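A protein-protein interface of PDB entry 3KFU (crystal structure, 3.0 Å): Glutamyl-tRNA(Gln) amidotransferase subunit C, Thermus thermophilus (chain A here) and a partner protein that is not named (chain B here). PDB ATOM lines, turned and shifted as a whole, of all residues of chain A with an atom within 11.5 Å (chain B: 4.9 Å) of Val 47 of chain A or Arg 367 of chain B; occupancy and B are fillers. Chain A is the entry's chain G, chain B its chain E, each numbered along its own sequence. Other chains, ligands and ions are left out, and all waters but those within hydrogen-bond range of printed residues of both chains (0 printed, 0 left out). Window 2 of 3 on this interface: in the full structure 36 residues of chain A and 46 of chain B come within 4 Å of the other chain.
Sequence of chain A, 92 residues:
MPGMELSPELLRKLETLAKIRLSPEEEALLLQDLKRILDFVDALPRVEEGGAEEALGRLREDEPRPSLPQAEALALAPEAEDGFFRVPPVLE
The backbone carbonyl oxygen of Gly 50 of chain A is in hydrogen-bond range of the guanidinium group of Arg 366 of chain B, at 3.2 Å.
NH1 of Arg 366 of chain B is in hydrogen-bond range of O of Gly 51 of chain A, at 2.6 Å.
OE2 of Glu 53 of chain A is in salt-bridge range of NH1 of Arg 366 of chain B (3.5 Å).
Among the printed residues, pairs that only touch across the chains: Leu 44 of chain A with Phe 364 of chain B (3.3 Å), Val 47 of chain A with Ala 363 of chain B (3.4 Å), Val 47 of chain A with Arg 367 of chain B (3.2 Å), Glu 49 of chain A with Ala 363 of chain B (3.6 Å) and Glu 49 of chain A with Arg 366 of chain B (3.0 Å).
Val 47 of chain A touches two residues of chain B.
Arg 367 of chain B touches just one residue of chain A: Val 47 (3.2 Å).
Ala 363 of chain B touches just these residues of chain A: Val 47 (3.4 Å) and Glu 49 (3.6 Å).
Ala 370 of chain B touches none of the printed residues of chain A.
No residue of chain A comes within 4 Å of Glu 371 of chain B.
Printed residues of chain B within 4 Å of Gly 51 of chain A: Arg 366 (2.6 Å).
Printed residues of chain B within 4 Å of Leu 44 of chain A: Phe 364 (3.3 Å).
Arg 46 of chain A touches none of the printed residues of chain B.
Arg 365 of chain B touches none of the printed residues of chain A.
The nearest residue of chain B that does not touch Val 47 of chain A is Phe 364 of chain B (4.6 Å).
The nearest residue of chain A that does not touch Arg 367 of chain B is Glu 48 of chain A (4.8 Å).
The nearest printed residue of chain B that does not touch Leu 44 of chain A is Arg 365 of chain B (6.9 Å).
Among the printed residues, 8 pairs touch across the chains.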
ATOM      1  N   VAL A  41     -27.294 -26.745 -10.625  1.00  0.00           N
ATOM      2  CA  VAL A  41     -26.338 -25.811 -10.046  1.00  0.00           C
ATOM      3  C   VAL A  41     -27.012 -24.813  -9.104  1.00  0.00           C
ATOM      4  O   VAL A  41     -26.481 -24.500  -8.040  1.00  0.00           O
ATOM      5  CB  VAL A  41     -25.574 -25.051 -11.152  1.00  0.00           C
ATOM      6  CG1 VAL A  41     -24.828 -23.857 -10.575  1.00  0.00           C
ATOM      7  CG2 VAL A  41     -24.621 -25.990 -11.874  1.00  0.00           C
ATOM      8  N   ASP A  42     -28.184 -24.324  -9.492  1.00  0.00           N
ATOM      9  CA  ASP A  42     -28.878 -23.305  -8.714  1.00  0.00           C
ATOM     10  C   ASP A  42     -29.229 -23.810  -7.318  1.00  0.00           C
ATOM     11  O   ASP A  42     -29.563 -23.024  -6.431  1.00  0.00           O
ATOM     12  CB  ASP A  42     -30.143 -22.843  -9.438  1.00  0.00           C
ATOM     13  CG  ASP A  42     -30.698 -21.550  -8.877  1.00  0.00           C
ATOM     14  OD1 ASP A  42     -29.895 -20.719  -8.400  1.00  0.00           O
ATOM     15  OD2 ASP A  42     -31.934 -21.364  -8.916  1.00  0.00           O
ATOM     16  N   ALA A  43     -29.150 -25.125  -7.132  1.00  0.00           N
ATOM     17  CA  ALA A  43     -29.440 -25.737  -5.839  1.00  0.00           C
ATOM     18  C   ALA A  43     -28.343 -25.434  -4.821  1.00  0.00           C
ATOM     19  O   ALA A  43     -28.492 -25.710  -3.630  1.00  0.00           O
ATOM     20  CB  ALA A  43     -29.621 -27.240  -5.993  1.00  0.00           C
ATOM     21  N   LEU A  44     -27.241 -24.871  -5.301  1.00  0.00           N
ATOM     22  CA  LEU A  44     -26.109 -24.528  -4.451  1.00  0.00           C
ATOM     23  C   LEU A  44     -26.524 -23.533  -3.371  1.00  0.00           C
ATOM     24  O   LEU A  44     -27.052 -22.465  -3.673  1.00  0.00           O
ATOM     25  CB  LEU A  44     -24.983 -23.928  -5.294  1.00  0.00           C
ATOM     26  CG  LEU A  44     -23.542 -24.344  -4.995  1.00  0.00           C
ATOM     27  CD1 LEU A  44     -22.578 -23.344  -5.610  1.00  0.00           C
ATOM     28  CD2 LEU A  44     -23.299 -24.459  -3.506  1.00  0.00           C
ATOM     29  N   PRO A  45     -26.295 -23.891  -2.103  1.00  0.00           N
ATOM     30  CA  PRO A  45     -26.567 -23.010  -0.962  1.00  0.00           C
ATOM     31  C   PRO A  45     -25.639 -21.801  -0.937  1.00  0.00           C
ATOM     32  O   PRO A  45     -24.483 -21.914  -1.342  1.00  0.00           O
ATOM     33  CB  PRO A  45     -26.265 -23.907   0.243  1.00  0.00           C
ATOM     34  CG  PRO A  45     -26.418 -25.296  -0.265  1.00  0.00           C
ATOM     35  CD  PRO A  45     -25.934 -25.252  -1.674  1.00  0.00           C
ATOM     36  N   ARG A  46     -26.134 -20.662  -0.463  1.00  0.00           N
ATOM     37  CA  ARG A  46     -25.276 -19.496  -0.290  1.00  0.00           C
ATOM     38  C   ARG A  46     -24.610 -19.499   1.079  1.00  0.00           C
ATOM     39  O   ARG A  46     -25.220 -19.875   2.078  1.00  0.00           O
ATOM     40  CB  ARG A  46     -26.045 -18.193  -0.494  1.00  0.00           C
ATOM     41  CG  ARG A  46     -25.198 -16.959  -0.214  1.00  0.00           C
ATOM     42  CD  ARG A  46     -25.627 -15.769  -1.048  1.00  0.00           C
ATOM     43  NE  ARG A  46     -24.464 -15.031  -1.528  1.00  0.00           N
ATOM     44  CZ  ARG A  46     -23.922 -15.193  -2.730  1.00  0.00           C
ATOM     45  NH1 ARG A  46     -24.452 -16.060  -3.583  1.00  0.00           N
ATOM     46  NH2 ARG A  46     -22.858 -14.485  -3.084  1.00  0.00           N
ATOM     47  N   VAL A  47     -23.356 -19.062   1.116  1.00  0.00           N
ATOM     48  CA  VAL A  47     -22.559 -19.100   2.331  1.00  0.00           C
ATOM     49  C   VAL A  47     -21.686 -17.855   2.465  1.00  0.00           C
ATOM     50  O   VAL A  47     -21.290 -17.253   1.467  1.00  0.00           O
ATOM     51  CB  VAL A  47     -21.666 -20.356   2.349  1.00  0.00           C
ATOM     52  CG1 VAL A  47     -20.574 -20.226   3.393  1.00  0.00           C
ATOM     53  CG2 VAL A  47     -22.507 -21.605   2.587  1.00  0.00           C
ATOM     54  N   GLU A  48     -21.395 -17.473   3.706  1.00  0.00           N
ATOM     55  CA  GLU A  48     -20.530 -16.332   3.991  1.00  0.00           C
ATOM     56  C   GLU A  48     -19.066 -16.657   3.693  1.00  0.00           C
ATOM     57  O   GLU A  48     -18.636 -17.802   3.835  1.00  0.00           O
ATOM     58  CB  GLU A  48     -20.684 -15.920   5.455  1.00  0.00           C
ATOM     59  CG  GLU A  48     -22.130 -15.765   5.898  1.00  0.00           C
ATOM     60  CD  GLU A  48     -22.312 -15.991   7.387  1.00  0.00           C
ATOM     61  OE1 GLU A  48     -21.296 -16.137   8.097  1.00  0.00           O
ATOM     62  OE2 GLU A  48     -23.474 -16.031   7.844  1.00  0.00           O
ATOM     63  N   GLU A  49     -18.304 -15.647   3.286  1.00  0.00           N
ATOM     64  CA  GLU A  49     -16.903 -15.844   2.923  1.00  0.00           C
ATOM     65  C   GLU A  49     -15.982 -14.943   3.745  1.00  0.00           C
ATOM     66  O   GLU A  49     -16.291 -13.776   3.975  1.00  0.00           O
ATOM     67  CB  GLU A  49     -16.706 -15.584   1.428  1.00  0.00           C
ATOM     68  CG  GLU A  49     -15.327 -15.943   0.902  1.00  0.00           C
ATOM     69  CD  GLU A  49     -15.219 -15.768  -0.600  1.00  0.00           C
ATOM     70  OE1 GLU A  49     -16.202 -15.304  -1.217  1.00  0.00           O
ATOM     71  OE2 GLU A  49     -14.154 -16.094  -1.165  1.00  0.00           O
ATOM     72  N   GLY A  50     -14.849 -15.486   4.180  1.00  0.00           N
ATOM     73  CA  GLY A  50     -13.942 -14.758   5.052  1.00  0.00           C
ATOM     74  C   GLY A  50     -12.913 -13.899   4.338  1.00  0.00           C
ATOM     75  O   GLY A  50     -12.989 -13.695   3.126  1.00  0.00           O
ATOM     76  N   GLY A  51     -11.948 -13.393   5.104  1.00  0.00           N
ATOM     77  CA  GLY A  51     -10.883 -12.561   4.569  1.00  0.00           C
ATOM     78  C   GLY A  51     -10.168 -13.215   3.404  1.00  0.00           C
ATOM     79  O   GLY A  51      -9.894 -14.412   3.428  1.00  0.00           O
ATOM     80  N   GLU A  53      -7.588 -14.295   2.152  1.00  0.00           N
ATOM     81  CA  GLU A  53      -6.293 -14.974   2.249  1.00  0.00           C
ATOM     82  C   GLU A  53      -5.109 -14.007   2.262  1.00  0.00           C
ATOM     83  O   GLU A  53      -5.269 -12.811   2.028  1.00  0.00           O
ATOM     84  CB  GLU A  53      -6.120 -15.983   1.104  1.00  0.00           C
ATOM     85  CG  GLU A  53      -7.404 -16.692   0.670  1.00  0.00           C
ATOM     86  CD  GLU A  53      -8.108 -15.991  -0.483  1.00  0.00           C
ATOM     87  OE1 GLU A  53      -7.470 -15.155  -1.159  1.00  0.00           O
ATOM     88  OE2 GLU A  53      -9.302 -16.277  -0.718  1.00  0.00           O
ATOM     89  N   SER B 286     -20.607 -30.341   3.693  1.00  0.00           N
ATOM     90  CA  SER B 286     -21.113 -29.850   2.413  1.00  0.00           C
ATOM     91  C   SER B 286     -20.496 -30.540   1.196  1.00  0.00           C
ATOM     92  O   SER B 286     -20.614 -30.058   0.071  1.00  0.00           O
ATOM     93  CB  SER B 286     -20.911 -28.338   2.319  1.00  0.00           C
ATOM     94  OG  SER B 286     -19.607 -27.980   2.737  1.00  0.00           O
ATOM     95  N   ALA B 363     -17.518 -18.583  -2.744  1.00  0.00           N
ATOM     96  CA  ALA B 363     -17.664 -18.594  -1.297  1.00  0.00           C
ATOM     97  C   ALA B 363     -17.809 -20.020  -0.785  1.00  0.00           C
ATOM     98  O   ALA B 363     -17.336 -20.352   0.301  1.00  0.00           O
ATOM     99  CB  ALA B 363     -18.859 -17.758  -0.879  1.00  0.00           C
ATOM    100  N   PHE B 364     -18.465 -20.859  -1.578  1.00  0.00           N
ATOM    101  CA  PHE B 364     -18.692 -22.246  -1.192  1.00  0.00           C
ATOM    102  C   PHE B 364     -17.401 -23.045  -1.300  1.00  0.00           C
ATOM    103  O   PHE B 364     -17.159 -23.963  -0.519  1.00  0.00           O
ATOM    104  CB  PHE B 364     -19.778 -22.873  -2.067  1.00  0.00           C
ATOM    105  CG  PHE B 364     -20.210 -24.237  -1.613  1.00  0.00           C
ATOM    106  CD1 PHE B 364     -21.327 -24.391  -0.813  1.00  0.00           C
ATOM    107  CD2 PHE B 364     -19.498 -25.366  -1.989  1.00  0.00           C
ATOM    108  CE1 PHE B 364     -21.730 -25.647  -0.397  1.00  0.00           C
ATOM    109  CE2 PHE B 364     -19.891 -26.623  -1.575  1.00  0.00           C
ATOM    110  CZ  PHE B 364     -21.010 -26.765  -0.778  1.00  0.00           C
ATOM    111  N   ARG B 365     -16.576 -22.693  -2.280  1.00  0.00           N
ATOM    112  CA  ARG B 365     -15.303 -23.367  -2.469  1.00  0.00           C
ATOM    113  C   ARG B 365     -14.420 -23.118  -1.257  1.00  0.00           C
ATOM    114  O   ARG B 365     -13.655 -23.989  -0.842  1.00  0.00           O
ATOM    115  CB  ARG B 365     -14.611 -22.874  -3.742  1.00  0.00           C
ATOM    116  CG  ARG B 365     -13.560 -23.839  -4.280  1.00  0.00           C
ATOM    117  CD  ARG B 365     -12.180 -23.207  -4.321  1.00  0.00           C
ATOM    118  NE  ARG B 365     -11.838 -22.702  -5.649  1.00  0.00           N
ATOM    119  CZ  ARG B 365     -11.071 -23.347  -6.521  1.00  0.00           C
ATOM    120  NH1 ARG B 365     -10.555 -24.525  -6.210  1.00  0.00           N
ATOM    121  NH2 ARG B 365     -10.812 -22.810  -7.705  1.00  0.00           N
ATOM    122  N   ARG B 366     -14.539 -21.926  -0.682  1.00  0.00           N
ATOM    123  CA  ARG B 366     -13.775 -21.577   0.511  1.00  0.00           C
ATOM    124  C   ARG B 366     -14.247 -22.330   1.763  1.00  0.00           C
ATOM    125  O   ARG B 366     -13.464 -22.564   2.684  1.00  0.00           O
ATOM    126  CB  ARG B 366     -13.807 -20.068   0.748  1.00  0.00           C
ATOM    127  CG  ARG B 366     -13.028 -19.267  -0.273  1.00  0.00           C
ATOM    128  CD  ARG B 366     -12.428 -18.026   0.359  1.00  0.00           C
ATOM    129  NE  ARG B 366     -11.363 -18.364   1.299  1.00  0.00           N
ATOM    130  CZ  ARG B 366     -10.836 -17.508   2.167  1.00  0.00           C
ATOM    131  NH1 ARG B 366     -11.282 -16.261   2.221  1.00  0.00           N
ATOM    132  NH2 ARG B 366      -9.869 -17.902   2.986  1.00  0.00           N
ATOM    133  N   ARG B 367     -15.523 -22.706   1.794  1.00  0.00           N
ATOM    134  CA  ARG B 367     -16.052 -23.528   2.879  1.00  0.00           C
ATOM    135  C   ARG B 367     -15.365 -24.881   2.918  1.00  0.00           C
ATOM    136  O   ARG B 367     -14.908 -25.323   3.969  1.00  0.00           O
ATOM    137  CB  ARG B 367     -17.555 -23.742   2.718  1.00  0.00           C
ATOM    138  CG  ARG B 367     -18.415 -22.776   3.498  1.00  0.00           C
ATOM    139  CD  ARG B 367     -18.504 -23.159   4.962  1.00  0.00           C
ATOM    140  NE  ARG B 367     -19.328 -22.211   5.709  1.00  0.00           N
ATOM    141  CZ  ARG B 367     -20.649 -22.297   5.822  1.00  0.00           C
ATOM    142  NH1 ARG B 367     -21.303 -23.292   5.237  1.00  0.00           N
ATOM    143  NH2 ARG B 367     -21.319 -21.386   6.515  1.00  0.00           N
ATOM    144  N   LEU B 368     -15.307 -25.541   1.767  1.00  0.00           N
ATOM    145  CA  LEU B 368     -14.715 -26.869   1.694  1.00  0.00           C
ATOM    146  C   LEU B 368     -13.295 -26.868   2.240  1.00  0.00           C
ATOM    147  O   LEU B 368     -12.937 -27.727   3.043  1.00  0.00           O
ATOM    148  CB  LEU B 368     -14.736 -27.409   0.264  1.00  0.00           C
ATOM    149  CG  LEU B 368     -16.102 -27.829  -0.273  1.00  0.00           C
ATOM    150  CD1 LEU B 368     -15.964 -28.341  -1.692  1.00  0.00           C
ATOM    151  CD2 LEU B 368     -16.725 -28.886   0.616  1.00  0.00           C
ATOM    152  N   LYS B 369     -12.490 -25.903   1.809  1.00  0.00           N
ATOM    153  CA  LYS B 369     -11.127 -25.796   2.309  1.00  0.00           C
ATOM    154  C   LYS B 369     -11.141 -25.693   3.826  1.00  0.00           C
ATOM    155  O   LYS B 369     -10.370 -26.366   4.510  1.00  0.00           O
ATOM    156  CB  LYS B 369     -10.405 -24.597   1.690  1.00  0.00           C
ATOM    157  CG  LYS B 369     -10.032 -24.797   0.229  1.00  0.00           C
ATOM    158  CD  LYS B 369      -9.290 -23.596  -0.337  1.00  0.00           C
ATOM    159  CE  LYS B 369      -9.016 -23.772  -1.827  1.00  0.00           C
ATOM    160  NZ  LYS B 369      -8.354 -22.582  -2.431  1.00  0.00           N
ATOM    161  N   ALA B 370     -12.037 -24.861   4.346  1.00  0.00           N
ATOM    162  CA  ALA B 370     -12.172 -24.682   5.786  1.00  0.00           C
ATOM    163  C   ALA B 370     -12.539 -25.992   6.476  1.00  0.00           C
ATOM    164  O   ALA B 370     -11.831 -26.452   7.372  1.00  0.00           O
ATOM    165  CB  ALA B 370     -13.211 -23.626   6.088  1.00  0.00           C
ATOM    166  N   GLU B 371     -13.651 -26.584   6.056  1.00  0.00           N
ATOM    167  CA  GLU B 371     -14.116 -27.835   6.637  1.00  0.00           C
ATOM    168  C   GLU B 371     -13.030 -28.907   6.577  1.00  0.00           C
ATOM    169  O   GLU B 371     -12.975 -29.800   7.423  1.00  0.00           O
ATOM    170  CB  GLU B 371     -15.385 -28.311   5.927  1.00  0.00           C
ATOM    171  CG  GLU B 371     -16.526 -27.313   5.973  1.00  0.00           C
ATOM    172  CD  GLU B 371     -17.824 -27.870   5.419  1.00  0.00           C
ATOM    173  OE1 GLU B 371     -17.789 -28.923   4.748  1.00  0.00           O
ATOM    174  OE2 GLU B 371     -18.883 -27.253   5.661  1.00  0.00           O
ATOM    175  N   ALA B 372     -12.167 -28.807   5.570  1.00  0.00           N
ATOM    176  CA  ALA B 372     -11.067 -29.747   5.400  1.00  0.00           C
ATOM    177  C   ALA B 372      -9.949 -29.466   6.395  1.00  0.00           C
ATOM    178  O   ALA B 372      -9.422 -30.389   7.014  1.00  0.00           O
ATOM    179  CB  ALA B 372     -10.537 -29.696   3.975  1.00  0.00           C
